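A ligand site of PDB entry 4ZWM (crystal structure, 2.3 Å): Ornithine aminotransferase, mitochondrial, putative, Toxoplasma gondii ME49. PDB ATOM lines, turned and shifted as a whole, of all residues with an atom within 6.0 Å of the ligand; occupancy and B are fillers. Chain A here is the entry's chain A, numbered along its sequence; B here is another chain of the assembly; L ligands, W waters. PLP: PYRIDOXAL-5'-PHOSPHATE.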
ATOM      1  N   VAL A  79       9.444   0.903   0.705  1.00  0.00           N
ATOM      2  CA  VAL A  79      10.661   1.455   1.232  1.00  0.00           C
ATOM      3  C   VAL A  79      11.495   1.897   0.015  1.00  0.00           C
ATOM      4  O   VAL A  79      12.657   1.480  -0.164  1.00  0.00           O
ATOM      5  CB  VAL A  79      11.417   0.435   2.113  1.00  0.00           C
ATOM      6  CG1 VAL A  79      12.411   1.143   3.027  1.00  0.00           C
ATOM      7  CG2 VAL A  79      10.481  -0.438   2.931  1.00  0.00           C
ATOM      8  N   ASN A 134      18.346 -10.443  -8.990  1.00  0.00           N
ATOM      9  CA  ASN A 134      16.907 -10.249  -8.804  1.00  0.00           C
ATOM     10  C   ASN A 134      16.625  -9.425  -7.553  1.00  0.00           C
ATOM     11  O   ASN A 134      15.928  -8.418  -7.650  1.00  0.00           O
ATOM     12  CB  ASN A 134      16.147 -11.573  -8.795  1.00  0.00           C
ATOM     13  CG  ASN A 134      16.536 -12.492  -9.942  1.00  0.00           C
ATOM     14  OD1 ASN A 134      15.987 -12.406 -11.023  1.00  0.00           O
ATOM     15  ND2 ASN A 134      17.478 -13.396  -9.696  1.00  0.00           N
ATOM     16  N   THR A 135      17.189  -9.821  -6.404  1.00  0.00           N
ATOM     17  CA  THR A 135      16.970  -9.114  -5.149  1.00  0.00           C
ATOM     18  C   THR A 135      18.119  -8.190  -4.710  1.00  0.00           C
ATOM     19  O   THR A 135      19.266  -8.382  -5.113  1.00  0.00           O
ATOM     20  CB  THR A 135      16.718 -10.114  -3.990  1.00  0.00           C
ATOM     21  OG1 THR A 135      17.926 -10.767  -3.620  1.00  0.00           O
ATOM     22  CG2 THR A 135      15.718 -11.173  -4.369  1.00  0.00           C
ATOM     23  N   GLY A 136      17.803  -7.234  -3.829  1.00  0.00           N
ATOM     24  CA  GLY A 136      18.814  -6.406  -3.131  1.00  0.00           C
ATOM     25  C   GLY A 136      19.896  -7.174  -2.374  1.00  0.00           C
ATOM     26  O   GLY A 136      21.091  -6.853  -2.443  1.00  0.00           O
ATOM     27  N   ALA A 137      19.447  -8.185  -1.643  1.00  0.00           N
ATOM     28  CA  ALA A 137      20.322  -9.081  -0.907  1.00  0.00           C
ATOM     29  C   ALA A 137      21.271  -9.801  -1.848  1.00  0.00           C
ATOM     30  O   ALA A 137      22.454  -9.867  -1.560  1.00  0.00           O
ATOM     31  CB  ALA A 137      19.500 -10.105  -0.124  1.00  0.00           C
ATOM     32  N   GLU A 138      20.759 -10.329  -2.945  1.00  0.00           N
ATOM     33  CA  GLU A 138      21.628 -10.989  -3.958  1.00  0.00           C
ATOM     34  C   GLU A 138      22.692 -10.025  -4.530  1.00  0.00           C
ATOM     35  O   GLU A 138      23.847 -10.414  -4.751  1.00  0.00           O
ATOM     36  CB  GLU A 138      20.818 -11.579  -5.120  1.00  0.00           C
ATOM     37  CG  GLU A 138      20.091 -12.864  -4.823  1.00  0.00           C
ATOM     38  CD  GLU A 138      19.402 -13.457  -6.073  1.00  0.00           C
ATOM     39  OE1 GLU A 138      19.232 -12.726  -7.078  1.00  0.00           O
ATOM     40  OE2 GLU A 138      19.020 -14.667  -6.041  1.00  0.00           O
ATOM     41  N   TYR A 171      21.742  -2.652   7.113  1.00  0.00           N
ATOM     42  CA  TYR A 171      20.776  -3.605   6.611  1.00  0.00           C
ATOM     43  C   TYR A 171      20.964  -3.720   5.096  1.00  0.00           C
ATOM     44  O   TYR A 171      20.737  -2.742   4.375  1.00  0.00           O
ATOM     45  CB  TYR A 171      19.329  -3.212   6.976  1.00  0.00           C
ATOM     46  CG  TYR A 171      18.328  -4.236   6.494  1.00  0.00           C
ATOM     47  CD1 TYR A 171      17.905  -4.247   5.133  1.00  0.00           C
ATOM     48  CD2 TYR A 171      17.841  -5.226   7.348  1.00  0.00           C
ATOM     49  CE1 TYR A 171      17.028  -5.210   4.675  1.00  0.00           C
ATOM     50  CE2 TYR A 171      16.958  -6.175   6.881  1.00  0.00           C
ATOM     51  CZ  TYR A 171      16.560  -6.156   5.539  1.00  0.00           C
ATOM     52  OH  TYR A 171      15.686  -7.091   5.089  1.00  0.00           O
ATOM     53  N   TRP A 172      21.371  -4.903   4.626  1.00  0.00           N
ATOM     54  CA  TRP A 172      21.411  -5.215   3.195  1.00  0.00           C
ATOM     55  C   TRP A 172      20.693  -6.497   2.773  1.00  0.00           C
ATOM     56  O   TRP A 172      20.732  -6.857   1.594  1.00  0.00           O
ATOM     57  CB  TRP A 172      22.858  -5.248   2.718  1.00  0.00           C
ATOM     58  CG  TRP A 172      23.751  -6.272   3.300  1.00  0.00           C
ATOM     59  CD1 TRP A 172      24.501  -6.165   4.439  1.00  0.00           C
ATOM     60  CD2 TRP A 172      24.045  -7.566   2.746  1.00  0.00           C
ATOM     61  NE1 TRP A 172      25.225  -7.326   4.638  1.00  0.00           N
ATOM     62  CE2 TRP A 172      24.956  -8.198   3.614  1.00  0.00           C
ATOM     63  CE3 TRP A 172      23.589  -8.262   1.624  1.00  0.00           C
ATOM     64  CZ2 TRP A 172      25.460  -9.475   3.378  1.00  0.00           C
ATOM     65  CZ3 TRP A 172      24.062  -9.548   1.405  1.00  0.00           C
ATOM     66  CH2 TRP A 172      25.002 -10.136   2.269  1.00  0.00           C
ATOM     67  N   GLY A 173      20.055  -7.202   3.711  1.00  0.00           N
ATOM     68  CA  GLY A 173      19.281  -8.359   3.373  1.00  0.00           C
ATOM     69  C   GLY A 173      19.155  -9.340   4.498  1.00  0.00           C
ATOM     70  O   GLY A 173      19.411  -9.005   5.645  1.00  0.00           O
ATOM     71  N   ARG A 174      18.730 -10.555   4.121  1.00  0.00           N
ATOM     72  CA  ARG A 174      18.295 -11.585   5.039  1.00  0.00           C
ATOM     73  C   ARG A 174      18.927 -12.949   4.783  1.00  0.00           C
ATOM     74  O   ARG A 174      18.569 -13.928   5.476  1.00  0.00           O
ATOM     75  CB  ARG A 174      16.789 -11.749   4.929  1.00  0.00           C
ATOM     76  CG  ARG A 174      16.009 -10.537   5.393  1.00  0.00           C
ATOM     77  CD  ARG A 174      16.038 -10.428   6.894  1.00  0.00           C
ATOM     78  NE  ARG A 174      15.097  -9.406   7.347  1.00  0.00           N
ATOM     79  CZ  ARG A 174      14.762  -9.192   8.609  1.00  0.00           C
ATOM     80  NH1 ARG A 174      15.306  -9.916   9.608  1.00  0.00           N
ATOM     81  NH2 ARG A 174      13.886  -8.233   8.893  1.00  0.00           N
ATOM     82  N   GLU A 224      26.123   2.396   3.438  1.00  0.00           N
ATOM     83  CA  GLU A 224      24.957   3.084   2.863  1.00  0.00           C
ATOM     84  C   GLU A 224      25.219   4.595   3.001  1.00  0.00           C
ATOM     85  O   GLU A 224      25.761   5.025   4.027  1.00  0.00           O
ATOM     86  CB  GLU A 224      23.632   2.670   3.570  1.00  0.00           C
ATOM     87  CG  GLU A 224      23.414   1.156   3.828  1.00  0.00           C
ATOM     88  CD  GLU A 224      22.299   0.787   4.854  1.00  0.00           C
ATOM     89  OE1 GLU A 224      21.087   1.150   4.652  1.00  0.00           O
ATOM     90  OE2 GLU A 224      22.647   0.106   5.865  1.00  0.00           O
ATOM     91  N   GLY A 228      19.180   3.216   5.945  1.00  0.00           N
ATOM     92  CA  GLY A 228      17.722   3.117   5.763  1.00  0.00           C
ATOM     93  C   GLY A 228      16.987   2.438   6.910  1.00  0.00           C
ATOM     94  O   GLY A 228      16.419   3.108   7.797  1.00  0.00           O
ATOM     95  N   GLU A 229      17.010   1.101   6.911  1.00  0.00           N
ATOM     96  CA  GLU A 229      16.334   0.353   7.983  1.00  0.00           C
ATOM     97  C   GLU A 229      16.929   0.660   9.370  1.00  0.00           C
ATOM     98  O   GLU A 229      16.242   0.484  10.354  1.00  0.00           O
ATOM     99  CB  GLU A 229      16.335  -1.170   7.751  1.00  0.00           C
ATOM    100  CG  GLU A 229      15.787  -1.659   6.411  1.00  0.00           C
ATOM    101  CD  GLU A 229      14.310  -1.299   6.148  1.00  0.00           C
ATOM    102  OE1 GLU A 229      13.440  -1.603   7.006  1.00  0.00           O
ATOM    103  OE2 GLU A 229      14.041  -0.735   5.052  1.00  0.00           O
ATOM    104  N   ASP A 257      25.856   0.921  -1.190  1.00  0.00           N
ATOM    105  CA  ASP A 257      24.535   0.353  -1.342  1.00  0.00           C
ATOM    106  C   ASP A 257      23.589   1.526  -1.548  1.00  0.00           C
ATOM    107  O   ASP A 257      23.374   2.330  -0.638  1.00  0.00           O
ATOM    108  CB  ASP A 257      24.144  -0.425  -0.069  1.00  0.00           C
ATOM    109  CG  ASP A 257      22.842  -1.147  -0.194  1.00  0.00           C
ATOM    110  OD1 ASP A 257      22.027  -0.788  -1.095  1.00  0.00           O
ATOM    111  OD2 ASP A 257      22.602  -2.086   0.616  1.00  0.00           O
ATOM    112  N   GLU A 258      23.096   1.642  -2.762  1.00  0.00           N
ATOM    113  CA  GLU A 258      22.094   2.656  -3.115  1.00  0.00           C
ATOM    114  C   GLU A 258      20.747   2.001  -3.411  1.00  0.00           C
ATOM    115  O   GLU A 258      19.936   2.554  -4.126  1.00  0.00           O
ATOM    116  CB  GLU A 258      22.611   3.454  -4.331  1.00  0.00           C
ATOM    117  CG  GLU A 258      23.884   4.211  -4.033  1.00  0.00           C
ATOM    118  CD  GLU A 258      23.717   5.713  -3.961  1.00  0.00           C
ATOM    119  OE1 GLU A 258      22.573   6.166  -3.702  1.00  0.00           O
ATOM    120  OE2 GLU A 258      24.729   6.465  -4.136  1.00  0.00           O
ATOM    121  N   ILE A 259      20.506   0.828  -2.843  1.00  0.00           N
ATOM    122  CA  ILE A 259      19.254   0.121  -3.085  1.00  0.00           C
ATOM    123  C   ILE A 259      18.064   0.942  -2.585  1.00  0.00           C
ATOM    124  O   ILE A 259      17.050   1.013  -3.247  1.00  0.00           O
ATOM    125  CB  ILE A 259      19.331  -1.323  -2.510  1.00  0.00           C
ATOM    126  CG1 ILE A 259      20.236  -2.165  -3.436  1.00  0.00           C
ATOM    127  CG2 ILE A 259      17.967  -1.941  -2.400  1.00  0.00           C
ATOM    128  CD1 ILE A 259      20.794  -3.456  -2.838  1.00  0.00           C
ATOM    129  N   GLN A 260      18.192   1.556  -1.422  1.00  0.00           N
ATOM    130  CA  GLN A 260      17.108   2.381  -0.876  1.00  0.00           C
ATOM    131  C   GLN A 260      17.311   3.880  -1.194  1.00  0.00           C
ATOM    132  O   GLN A 260      16.351   4.592  -1.471  1.00  0.00           O
ATOM    133  CB  GLN A 260      16.986   2.138   0.636  1.00  0.00           C
ATOM    134  CG  GLN A 260      16.047   3.111   1.373  1.00  0.00           C
ATOM    135  CD  GLN A 260      15.508   2.611   2.717  1.00  0.00           C
ATOM    136  OE1 GLN A 260      14.713   3.313   3.362  1.00  0.00           O
ATOM    137  NE2 GLN A 260      15.926   1.398   3.150  1.00  0.00           N
ATOM    138  N   THR A 261      18.563   4.331  -1.148  1.00  0.00           N
ATOM    139  CA  THR A 261      18.908   5.744  -1.370  1.00  0.00           C
ATOM    140  C   THR A 261      19.067   6.180  -2.816  1.00  0.00           C
ATOM    141  O   THR A 261      19.058   7.374  -3.069  1.00  0.00           O
ATOM    142  CB  THR A 261      20.217   6.138  -0.639  1.00  0.00           C
ATOM    143  OG1 THR A 261      21.347   5.484  -1.237  1.00  0.00           O
ATOM    144  CG2 THR A 261      20.149   5.797   0.846  1.00  0.00           C
ATOM    145  N   LYS A 286      15.315  -2.175  -5.842  1.00  0.00           N
ATOM    146  CA  LYS A 286      14.026  -1.550  -5.556  1.00  0.00           C
ATOM    147  C   LYS A 286      13.562  -0.769  -6.792  1.00  0.00           C
ATOM    148  O   LYS A 286      13.262  -1.381  -7.783  1.00  0.00           O
ATOM    149  CB  LYS A 286      14.161  -0.703  -4.289  1.00  0.00           C
ATOM    150  CG  LYS A 286      14.284  -1.518  -3.018  1.00  0.00           C
ATOM    151  CD  LYS A 286      13.914  -0.662  -1.823  1.00  0.00           C
ATOM    152  CE  LYS A 286      14.476  -1.135  -0.489  1.00  0.00           C
ATOM    153  NZ  LYS A 286      13.527  -2.008   0.245  1.00  0.00           N
ATOM    154  N   ASN B 134      11.658 -14.833  -3.646  1.00  0.00           N
ATOM    155  CA  ASN B 134      11.787 -14.497  -5.062  1.00  0.00           C
ATOM    156  C   ASN B 134      12.592 -15.511  -5.828  1.00  0.00           C
ATOM    157  O   ASN B 134      12.114 -16.024  -6.829  1.00  0.00           O
ATOM    158  CB  ASN B 134      12.406 -13.116  -5.225  1.00  0.00           C
ATOM    159  CG  ASN B 134      11.663 -12.064  -4.447  1.00  0.00           C
ATOM    160  OD1 ASN B 134      10.530 -11.698  -4.771  1.00  0.00           O
ATOM    161  ND2 ASN B 134      12.282 -11.581  -3.408  1.00  0.00           N
ATOM    162  N   GLU B 138      17.150 -18.021  -2.391  1.00  0.00           N
ATOM    163  CA  GLU B 138      16.471 -17.480  -1.180  1.00  0.00           C
ATOM    164  C   GLU B 138      15.608 -18.499  -0.431  1.00  0.00           C
ATOM    165  O   GLU B 138      15.541 -18.494   0.795  1.00  0.00           O
ATOM    166  CB  GLU B 138      15.617 -16.255  -1.527  1.00  0.00           C
ATOM    167  CG  GLU B 138      16.460 -15.006  -1.580  1.00  0.00           C
ATOM    168  CD  GLU B 138      15.694 -13.757  -1.986  1.00  0.00           C
ATOM    169  OE1 GLU B 138      14.476 -13.855  -2.365  1.00  0.00           O
ATOM    170  OE2 GLU B 138      16.392 -12.690  -1.888  1.00  0.00           O
ATOM    171  N   GLY B 314      12.421 -11.646   6.114  1.00  0.00           N
ATOM    172  CA  GLY B 314      11.653 -10.838   5.165  1.00  0.00           C
ATOM    173  C   GLY B 314      12.316 -10.730   3.787  1.00  0.00           C
ATOM    174  O   GLY B 314      13.267 -11.445   3.480  1.00  0.00           O
ATOM    175  N   SER B 315      11.794  -9.813   2.976  1.00  0.00           N
ATOM    176  CA  SER B 315      12.205  -9.594   1.571  1.00  0.00           C
ATOM    177  C   SER B 315      11.305  -8.492   1.025  1.00  0.00           C
ATOM    178  O   SER B 315      10.132  -8.464   1.322  1.00  0.00           O
ATOM    179  CB  SER B 315      12.052 -10.885   0.735  1.00  0.00           C
ATOM    180  OG  SER B 315      11.776 -10.678  -0.666  1.00  0.00           O
ATOM    181  N   THR B 316      11.855  -7.570   0.253  1.00  0.00           N
ATOM    182  CA  THR B 316      11.037  -6.501  -0.336  1.00  0.00           C
ATOM    183  C   THR B 316       9.976  -7.113  -1.250  1.00  0.00           C
ATOM    184  O   THR B 316       8.771  -6.818  -1.113  1.00  0.00           O
ATOM    185  CB  THR B 316      11.905  -5.496  -1.109  1.00  0.00           C
ATOM    186  OG1 THR B 316      12.864  -4.916  -0.208  1.00  0.00           O
ATOM    187  CG2 THR B 316      11.039  -4.372  -1.754  1.00  0.00           C
ATOM    188  N   PHE B 317      10.397  -7.987  -2.155  1.00  0.00           N
ATOM    189  CA  PHE B 317       9.474  -8.502  -3.179  1.00  0.00           C
ATOM    190  C   PHE B 317       8.824  -9.856  -2.921  1.00  0.00           C
ATOM    191  O   PHE B 317       7.932 -10.255  -3.670  1.00  0.00           O
ATOM    192  CB  PHE B 317      10.163  -8.555  -4.533  1.00  0.00           C
ATOM    193  CG  PHE B 317      10.401  -7.212  -5.126  1.00  0.00           C
ATOM    194  CD1 PHE B 317       9.446  -6.630  -5.913  1.00  0.00           C
ATOM    195  CD2 PHE B 317      11.600  -6.557  -4.911  1.00  0.00           C
ATOM    196  CE1 PHE B 317       9.655  -5.387  -6.476  1.00  0.00           C
ATOM    197  CE2 PHE B 317      11.825  -5.306  -5.460  1.00  0.00           C
ATOM    198  CZ  PHE B 317      10.840  -4.711  -6.243  1.00  0.00           C
HETATM  199  N1  PLP L   1      19.944  -2.936   0.811  1.00  0.00           N
HETATM  200  C2  PLP L   1      19.246  -1.939   1.430  1.00  0.00           C
HETATM  201  C2A PLP L   1      19.946  -0.644   1.759  1.00  0.00           C
HETATM  202  C3  PLP L   1      17.812  -2.140   1.782  1.00  0.00           C
HETATM  203  O3  PLP L   1      17.067  -1.195   2.416  1.00  0.00           O
HETATM  204  C4  PLP L   1      17.215  -3.439   1.421  1.00  0.00           C
HETATM  205  C4A PLP L   1      15.802  -3.703   1.763  1.00  0.00           C
HETATM  206  C5  PLP L   1      18.089  -4.429   0.742  1.00  0.00           C
HETATM  207  C6  PLP L   1      19.416  -4.118   0.467  1.00  0.00           C
HETATM  208  C5A PLP L   1      17.561  -5.782   0.356  1.00  0.00           C
HETATM  209  O4P PLP L   1      16.632  -5.647  -0.727  1.00  0.00           O
HETATM  210  P   PLP L   1      15.640  -6.875  -0.981  1.00  0.00           P
HETATM  211  O1P PLP L   1      14.644  -6.701   0.124  1.00  0.00           O
HETATM  212  O2P PLP L   1      16.471  -8.137  -0.814  1.00  0.00           O
HETATM  213  O3P PLP L   1      15.161  -6.618  -2.399  1.00  0.00           O
HETATM  214  O   HOH W   1      16.322 -10.286   1.692  1.00  0.00           O
HETATM  215  O   HOH W   2      18.667  -0.477   4.717  1.00  0.00           O
HETATM  216  O   HOH W   3      13.233  -8.639  -2.609  1.00  0.00           O
HETATM  217  O   HOH W   4      14.746 -10.645  -1.006  1.00  0.00           O
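The side-chain hydroxyl (OG1) of Thr 316 of chain B lies within hydrogen-bond range of an oxygen (O1P) of the ligand. The side-chain carboxylate (OD2) of Asp 257 is in hydrogen-bond range of a nitrogen (N1) of the ligand (2.8 Å). An oxygen (O3P) of the ligand sits at hydrogen-bond distance from the backbone NH (N) of Gly 136 (3.1 Å). NE2 of Gln 260 sits at hydrogen-bond distance from O3 of the ligand, 2.9 Å away. The backbone NH of Thr 316 of chain B is in hydrogen-bond range of an oxygen (O1P) of the ligand, 2.9 Å away. N of Ala 137 is in hydrogen-bond range of O2P of the ligand (3.1 Å).
The backbone NH (N) of Tyr 171 lies within hydrogen-bond range of the side-chain carboxylate (OE2) of Glu 224, at 3.2 Å. OD1 of Asp 257 is in hydrogen-bond range of N of Ile 259 (2.8 Å). OG1 of Thr 135 lies close to OE2 of Glu 138 of chain B (3.0 Å). N of Glu 138 of chain A is in hydrogen-bond range of OG1 of Thr 135 (2.9 Å). The side-chain hydroxyl of Ser 315 of chain B sits close to the backbone NH of Phe 317 of chain B, at 3.4 Å. The side-chain hydroxyl (OG) of Ser 315 of chain B is in hydrogen-bond range of the side-chain amide nitrogen (ND2) of Asn 134 of chain B (2.9 Å). NE of Arg 174 lies within hydrogen-bond range of OH of Tyr 171 (3.3 Å). OE1 of Glu 224 sits at hydrogen-bond distance from N of Gly 228 (3.1 Å).
Merely in contact with the ligand: Lys 286 (3.2 Å), Trp 172 (3.2 Å), Tyr 171 (3.4 Å), Glu 224 (3.6 Å), Ile 259 (3.6 Å), Thr 135 (3.7 Å) and Ser 315 of chain B (3.9 Å). Hydrophobic or aromatic side chains that line the ligand: Ala 137, Tyr 171 and Ile 259. 12 residues have an atom within 4 Å of the ligand: Thr 135, Gly 136, Ala 137, Tyr 171, Trp 172, Glu 224, Asp 257, Ile 259, Gln 260, Lys 286, Ser 315 of chain B and Thr 316 of chain B.
Water W2 lies within hydrogen-bond range of an oxygen (O3) of the ligand, the side-chain carboxylate of Glu 224, the backbone carbonyl oxygen of Tyr 171 and the backbone NH of Glu 229. Water W4 lies within hydrogen-bond range of the side-chain carboxylate (OE2) of Glu 138 of chain B (2.8 Å), the side-chain hydroxyl (OG) of Ser 315 of chain B (3.0 Å) and an oxygen (O2P) of the ligand (3.1 Å). Water W1 bridges an oxygen (O2P) of the ligand and the backbone NH of Arg 174.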
